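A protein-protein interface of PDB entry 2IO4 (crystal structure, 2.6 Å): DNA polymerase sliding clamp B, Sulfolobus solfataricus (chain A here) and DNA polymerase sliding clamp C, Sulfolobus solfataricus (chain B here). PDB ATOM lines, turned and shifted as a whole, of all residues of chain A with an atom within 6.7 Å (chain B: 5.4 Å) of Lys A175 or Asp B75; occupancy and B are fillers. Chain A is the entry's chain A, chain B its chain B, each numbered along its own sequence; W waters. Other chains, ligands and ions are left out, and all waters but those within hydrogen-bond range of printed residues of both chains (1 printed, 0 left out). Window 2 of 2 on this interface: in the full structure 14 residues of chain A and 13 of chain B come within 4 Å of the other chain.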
ATOM      1  N   LEU A 152       8.235 -29.034 -21.979  1.00  0.00           N
ATOM      2  CA  LEU A 152       9.070 -28.792 -20.801  1.00  0.00           C
ATOM      3  C   LEU A 152      10.134 -27.714 -21.062  1.00  0.00           C
ATOM      4  O   LEU A 152      10.600 -27.054 -20.131  1.00  0.00           O
ATOM      5  CB  LEU A 152       9.726 -30.104 -20.328  1.00  0.00           C
ATOM      6  CG  LEU A 152      10.981 -30.068 -19.428  1.00  0.00           C
ATOM      7  CD1 LEU A 152      10.686 -29.598 -17.993  1.00  0.00           C
ATOM      8  CD2 LEU A 152      11.699 -31.410 -19.414  1.00  0.00           C
ATOM      9  N   VAL A 153      10.501 -27.517 -22.325  1.00  0.00           N
ATOM     10  CA  VAL A 153      11.635 -26.639 -22.634  1.00  0.00           C
ATOM     11  C   VAL A 153      11.261 -25.337 -23.374  1.00  0.00           C
ATOM     12  O   VAL A 153      11.941 -24.317 -23.222  1.00  0.00           O
ATOM     13  CB  VAL A 153      12.793 -27.415 -23.349  1.00  0.00           C
ATOM     14  CG1 VAL A 153      13.990 -26.531 -23.542  1.00  0.00           C
ATOM     15  CG2 VAL A 153      13.209 -28.642 -22.533  1.00  0.00           C
ATOM     16  N   GLY A 154      10.181 -25.357 -24.147  1.00  0.00           N
ATOM     17  CA  GLY A 154       9.798 -24.176 -24.931  1.00  0.00           C
ATOM     18  C   GLY A 154       8.347 -24.143 -25.362  1.00  0.00           C
ATOM     19  O   GLY A 154       7.594 -25.095 -25.123  1.00  0.00           O
ATOM     20  N   ALA A 170      13.755 -27.552 -29.462  1.00  0.00           N
ATOM     21  CA  ALA A 170      13.045 -26.470 -28.760  1.00  0.00           C
ATOM     22  C   ALA A 170      13.923 -25.810 -27.678  1.00  0.00           C
ATOM     23  O   ALA A 170      14.973 -26.340 -27.316  1.00  0.00           O
ATOM     24  CB  ALA A 170      11.728 -26.978 -28.166  1.00  0.00           C
ATOM     25  N   GLY A 171      13.482 -24.655 -27.172  1.00  0.00           N
ATOM     26  CA  GLY A 171      14.234 -23.874 -26.187  1.00  0.00           C
ATOM     27  C   GLY A 171      14.692 -22.548 -26.776  1.00  0.00           C
ATOM     28  O   GLY A 171      15.505 -22.522 -27.716  1.00  0.00           O
ATOM     29  N   GLU A 172      14.176 -21.444 -26.227  1.00  0.00           N
ATOM     30  CA  GLU A 172      14.403 -20.107 -26.817  1.00  0.00           C
ATOM     31  C   GLU A 172      15.620 -19.377 -26.253  1.00  0.00           C
ATOM     32  O   GLU A 172      16.228 -18.561 -26.957  1.00  0.00           O
ATOM     33  CB  GLU A 172      13.144 -19.216 -26.715  1.00  0.00           C
ATOM     34  CG  GLU A 172      13.172 -18.109 -25.623  1.00  0.00           C
ATOM     35  CD  GLU A 172      12.498 -18.502 -24.294  1.00  0.00           C
ATOM     36  OE1 GLU A 172      12.149 -19.698 -24.093  1.00  0.00           O
ATOM     37  OE2 GLU A 172      12.322 -17.596 -23.441  1.00  0.00           O
ATOM     38  N   GLU A 173      15.962 -19.670 -24.993  1.00  0.00           N
ATOM     39  CA  GLU A 173      17.017 -18.941 -24.287  1.00  0.00           C
ATOM     40  C   GLU A 173      18.359 -19.698 -24.287  1.00  0.00           C
ATOM     41  O   GLU A 173      19.178 -19.501 -25.187  1.00  0.00           O
ATOM     42  CB  GLU A 173      16.564 -18.597 -22.861  1.00  0.00           C
ATOM     43  CG  GLU A 173      17.370 -17.482 -22.216  1.00  0.00           C
ATOM     44  CD  GLU A 173      17.166 -17.420 -20.705  1.00  0.00           C
ATOM     45  OE1 GLU A 173      16.323 -18.180 -20.164  1.00  0.00           O
ATOM     46  OE2 GLU A 173      17.855 -16.604 -20.054  1.00  0.00           O
ATOM     47  N   GLY A 174      18.572 -20.552 -23.281  1.00  0.00           N
ATOM     48  CA  GLY A 174      19.788 -21.373 -23.175  1.00  0.00           C
ATOM     49  C   GLY A 174      19.491 -22.850 -22.956  1.00  0.00           C
ATOM     50  O   GLY A 174      20.276 -23.722 -23.402  1.00  0.00           O
ATOM     51  N   LYS A 175      18.358 -23.118 -22.263  1.00  0.00           N
ATOM     52  CA  LYS A 175      17.900 -24.480 -21.955  1.00  0.00           C
ATOM     53  C   LYS A 175      17.271 -25.102 -23.195  1.00  0.00           C
ATOM     54  O   LYS A 175      16.323 -24.544 -23.757  1.00  0.00           O
ATOM     55  CB  LYS A 175      16.872 -24.465 -20.812  1.00  0.00           C
ATOM     56  CG  LYS A 175      17.380 -23.907 -19.477  1.00  0.00           C
ATOM     57  CD  LYS A 175      16.259 -23.921 -18.430  1.00  0.00           C
ATOM     58  CE  LYS A 175      16.762 -23.247 -17.115  1.00  0.00           C
ATOM     59  NZ  LYS A 175      15.602 -23.173 -16.156  1.00  0.00           N
ATOM     60  N   ARG A 176      17.775 -26.264 -23.609  1.00  0.00           N
ATOM     61  CA  ARG A 176      17.474 -26.787 -24.943  1.00  0.00           C
ATOM     62  C   ARG A 176      17.128 -28.286 -24.993  1.00  0.00           C
ATOM     63  O   ARG A 176      17.379 -29.019 -24.036  1.00  0.00           O
ATOM     64  CB  ARG A 176      18.649 -26.466 -25.864  1.00  0.00           C
ATOM     65  CG  ARG A 176      18.243 -25.742 -27.129  1.00  0.00           C
ATOM     66  CD  ARG A 176      19.333 -24.791 -27.597  1.00  0.00           C
ATOM     67  NE  ARG A 176      20.603 -25.473 -27.868  1.00  0.00           N
ATOM     68  CZ  ARG A 176      20.867 -26.193 -28.964  1.00  0.00           C
ATOM     69  NH1 ARG A 176      19.942 -26.356 -29.906  1.00  0.00           N
ATOM     70  NH2 ARG A 176      22.064 -26.759 -29.116  1.00  0.00           N
ATOM     71  N   TYR A 177      16.544 -28.723 -26.114  1.00  0.00           N
ATOM     72  CA  TYR A 177      16.163 -30.128 -26.347  1.00  0.00           C
ATOM     73  C   TYR A 177      16.369 -30.539 -27.805  1.00  0.00           C
ATOM     74  O   TYR A 177      15.925 -29.828 -28.714  1.00  0.00           O
ATOM     75  CB  TYR A 177      14.688 -30.346 -25.978  1.00  0.00           C
ATOM     76  CG  TYR A 177      14.104 -31.685 -26.410  1.00  0.00           C
ATOM     77  CD1 TYR A 177      14.488 -32.875 -25.771  1.00  0.00           C
ATOM     78  CD2 TYR A 177      13.163 -31.758 -27.444  1.00  0.00           C
ATOM     79  CE1 TYR A 177      13.957 -34.100 -26.155  1.00  0.00           C
ATOM     80  CE2 TYR A 177      12.621 -32.983 -27.842  1.00  0.00           C
ATOM     81  CZ  TYR A 177      13.026 -34.146 -27.194  1.00  0.00           C
ATOM     82  OH  TYR A 177      12.489 -35.357 -27.567  1.00  0.00           O
ATOM     83  N   LYS B  72      21.296 -26.622 -11.248  1.00  0.00           N
ATOM     84  CA  LYS B  72      20.121 -26.471 -10.408  1.00  0.00           C
ATOM     85  C   LYS B  72      19.514 -27.861 -10.260  1.00  0.00           C
ATOM     86  O   LYS B  72      19.540 -28.655 -11.205  1.00  0.00           O
ATOM     87  CB  LYS B  72      19.125 -25.507 -11.056  1.00  0.00           C
ATOM     88  CG  LYS B  72      18.060 -24.976 -10.118  1.00  0.00           C
ATOM     89  CD  LYS B  72      17.205 -23.916 -10.784  1.00  0.00           C
ATOM     90  CE  LYS B  72      16.023 -23.551  -9.903  1.00  0.00           C
ATOM     91  NZ  LYS B  72      15.438 -22.239 -10.292  1.00  0.00           N
ATOM     92  N   LEU B  73      18.975 -28.167  -9.086  1.00  0.00           N
ATOM     93  CA  LEU B  73      18.406 -29.494  -8.864  1.00  0.00           C
ATOM     94  C   LEU B  73      17.041 -29.694  -9.506  1.00  0.00           C
ATOM     95  O   LEU B  73      16.757 -30.768 -10.039  1.00  0.00           O
ATOM     96  CB  LEU B  73      18.387 -29.835  -7.379  1.00  0.00           C
ATOM     97  CG  LEU B  73      19.669 -30.597  -7.047  1.00  0.00           C
ATOM     98  CD1 LEU B  73      20.111 -30.334  -5.641  1.00  0.00           C
ATOM     99  CD2 LEU B  73      19.496 -32.090  -7.280  1.00  0.00           C
ATOM    100  N   GLU B  74      16.209 -28.658  -9.454  1.00  0.00           N
ATOM    101  CA  GLU B  74      14.908 -28.668 -10.113  1.00  0.00           C
ATOM    102  C   GLU B  74      15.046 -28.888 -11.625  1.00  0.00           C
ATOM    103  O   GLU B  74      14.323 -29.699 -12.214  1.00  0.00           O
ATOM    104  CB  GLU B  74      14.179 -27.351  -9.849  1.00  0.00           C
ATOM    105  CG  GLU B  74      13.239 -27.370  -8.654  1.00  0.00           C
ATOM    106  CD  GLU B  74      11.972 -26.552  -8.911  1.00  0.00           C
ATOM    107  OE1 GLU B  74      10.860 -27.069  -8.646  1.00  0.00           O
ATOM    108  OE2 GLU B  74      12.085 -25.400  -9.399  1.00  0.00           O
ATOM    109  N   ASP B  75      15.987 -28.170 -12.238  1.00  0.00           N
ATOM    110  CA  ASP B  75      16.190 -28.234 -13.684  1.00  0.00           C
ATOM    111  C   ASP B  75      16.659 -29.615 -14.144  1.00  0.00           C
ATOM    112  O   ASP B  75      16.167 -30.138 -15.151  1.00  0.00           O
ATOM    113  CB  ASP B  75      17.132 -27.120 -14.163  1.00  0.00           C
ATOM    114  CG  ASP B  75      16.514 -25.726 -14.027  1.00  0.00           C
ATOM    115  OD1 ASP B  75      15.304 -25.604 -13.737  1.00  0.00           O
ATOM    116  OD2 ASP B  75      17.245 -24.734 -14.215  1.00  0.00           O
ATOM    117  N   VAL B  76      17.579 -30.210 -13.393  1.00  0.00           N
ATOM    118  CA  VAL B  76      18.036 -31.566 -13.673  1.00  0.00           C
ATOM    119  C   VAL B  76      16.937 -32.579 -13.393  1.00  0.00           C
ATOM    120  O   VAL B  76      16.737 -33.513 -14.177  1.00  0.00           O
ATOM    121  CB  VAL B  76      19.267 -31.943 -12.839  1.00  0.00           C
ATOM    122  CG1 VAL B  76      19.544 -33.440 -12.940  1.00  0.00           C
ATOM    123  CG2 VAL B  76      20.477 -31.149 -13.290  1.00  0.00           C
ATOM    124  N   ASN B  77      16.232 -32.404 -12.275  1.00  0.00           N
ATOM    125  CA  ASN B  77      15.195 -33.359 -11.906  1.00  0.00           C
ATOM    126  C   ASN B  77      13.961 -33.294 -12.795  1.00  0.00           C
ATOM    127  O   ASN B  77      13.326 -34.317 -13.055  1.00  0.00           O
ATOM    128  CB  ASN B  77      14.823 -33.227 -10.431  1.00  0.00           C
ATOM    129  CG  ASN B  77      15.791 -33.958  -9.515  1.00  0.00           C
ATOM    130  OD1 ASN B  77      16.308 -35.030  -9.854  1.00  0.00           O
ATOM    131  ND2 ASN B  77      16.028 -33.387  -8.338  1.00  0.00           N
ATOM    132  N   ASP B  78      13.628 -32.099 -13.268  1.00  0.00           N
ATOM    133  CA  ASP B  78      12.540 -31.973 -14.228  1.00  0.00           C
ATOM    134  C   ASP B  78      12.878 -32.801 -15.463  1.00  0.00           C
ATOM    135  O   ASP B  78      12.032 -33.539 -15.960  1.00  0.00           O
ATOM    136  CB  ASP B  78      12.278 -30.511 -14.601  1.00  0.00           C
ATOM    137  CG  ASP B  78      11.499 -29.747 -13.522  1.00  0.00           C
ATOM    138  OD1 ASP B  78      10.823 -30.364 -12.660  1.00  0.00           O
ATOM    139  OD2 ASP B  78      11.563 -28.501 -13.545  1.00  0.00           O
ATOM    140  N   ILE B  79      14.127 -32.706 -15.925  1.00  0.00           N
ATOM    141  CA  ILE B  79      14.612 -33.511 -17.050  1.00  0.00           C
ATOM    142  C   ILE B  79      14.552 -35.016 -16.759  1.00  0.00           C
ATOM    143  O   ILE B  79      14.009 -35.779 -17.557  1.00  0.00           O
ATOM    144  CB  ILE B  79      16.032 -33.082 -17.494  1.00  0.00           C
ATOM    145  CG1 ILE B  79      15.970 -31.714 -18.184  1.00  0.00           C
ATOM    146  CG2 ILE B  79      16.647 -34.124 -18.423  1.00  0.00           C
ATOM    147  CD1 ILE B  79      17.254 -30.915 -18.104  1.00  0.00           C
ATOM    148  N   GLU B 111      19.665 -30.032 -22.723  1.00  0.00           N
ATOM    149  CA  GLU B 111      20.830 -29.211 -22.427  1.00  0.00           C
ATOM    150  C   GLU B 111      20.585 -28.221 -21.301  1.00  0.00           C
ATOM    151  O   GLU B 111      19.564 -27.532 -21.271  1.00  0.00           O
ATOM    152  CB  GLU B 111      21.277 -28.462 -23.677  1.00  0.00           C
ATOM    153  CG  GLU B 111      21.748 -29.370 -24.799  1.00  0.00           C
ATOM    154  CD  GLU B 111      22.457 -28.616 -25.909  1.00  0.00           C
ATOM    155  OE1 GLU B 111      21.944 -27.560 -26.347  1.00  0.00           O
ATOM    156  OE2 GLU B 111      23.532 -29.091 -26.344  1.00  0.00           O
ATOM    157  N   LEU B 112      21.533 -28.152 -20.371  1.00  0.00           N
ATOM    158  CA  LEU B 112      21.503 -27.122 -19.345  1.00  0.00           C
ATOM    159  C   LEU B 112      22.809 -26.341 -19.361  1.00  0.00           C
ATOM    160  O   LEU B 112      23.881 -26.929 -19.164  1.00  0.00           O
ATOM    161  CB  LEU B 112      21.253 -27.715 -17.950  1.00  0.00           C
ATOM    162  CG  LEU B 112      19.898 -28.362 -17.641  1.00  0.00           C
ATOM    163  CD1 LEU B 112      19.962 -29.051 -16.300  1.00  0.00           C
ATOM    164  CD2 LEU B 112      18.737 -27.364 -17.673  1.00  0.00           C
ATOM    165  N   PRO B 113      22.724 -25.016 -19.610  1.00  0.00           N
ATOM    166  CA  PRO B 113      23.897 -24.159 -19.474  1.00  0.00           C
ATOM    167  C   PRO B 113      24.423 -24.294 -18.057  1.00  0.00           C
ATOM    168  O   PRO B 113      23.626 -24.374 -17.105  1.00  0.00           O
ATOM    169  CB  PRO B 113      23.338 -22.749 -19.686  1.00  0.00           C
ATOM    170  CG  PRO B 113      22.090 -22.941 -20.463  1.00  0.00           C
ATOM    171  CD  PRO B 113      21.522 -24.255 -20.015  1.00  0.00           C
HETATM  172  O   HOH W   1      22.216 -25.462 -24.743  1.00  0.00           O
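Among the printed residues, merely in contact across the chains: Leu A152 with Asp B78 (3.9 Å), Gly A174 with Pro B113 (3.5 Å) and Lys A175 with Glu B111 (3.5 Å).
Water W1 bridges the side-chain carboxylate (OE1) of Glu B111 and the backbone carbonyl oxygen (O) of Gly A174.
Of the 11 printed residues of chain B, 4 touch a printed residue of chain A. Printed residues of chain B that touch a printed residue of chain A: Asp B75, Asp B78, Glu B111 and Pro B113. Hydrophobic or aromatic side chains of chain B within 4 Å of the printed part of chain A: Pro B113. Of the 11 printed residues of chain A, 4 touch a printed residue of chain B. Among the printed residues, 5 pairs touch across the chains. Among the printed residues, Asp or Glu carboxylates within 4 Å of a Lys or Arg side-chain nitrogen of the other chain: Lys A175 with Asp B75 (3.0 Å) and Arg A176 with Glu B111 (2.9 Å).
Of the printed residues of chain B, Gly A174 touches Pro B113 (3.5 Å). Printed residues of chain B within 4 Å of Arg A176: Glu B111 (2.8 Å). Asp B75 touches just one residue of chain A: Lys A175 (3.0 Å). The nearest residue of chain A that does not touch Asp B75 is Leu A152 (6.2 Å).
The side-chain carboxylate (OD2) of Asp B75 is in salt-bridge range of the side-chain amino group (NZ) of Lys A175 (3.0 Å). NH2 of Arg A176 is in salt-bridge range of OE1 of Glu B111.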
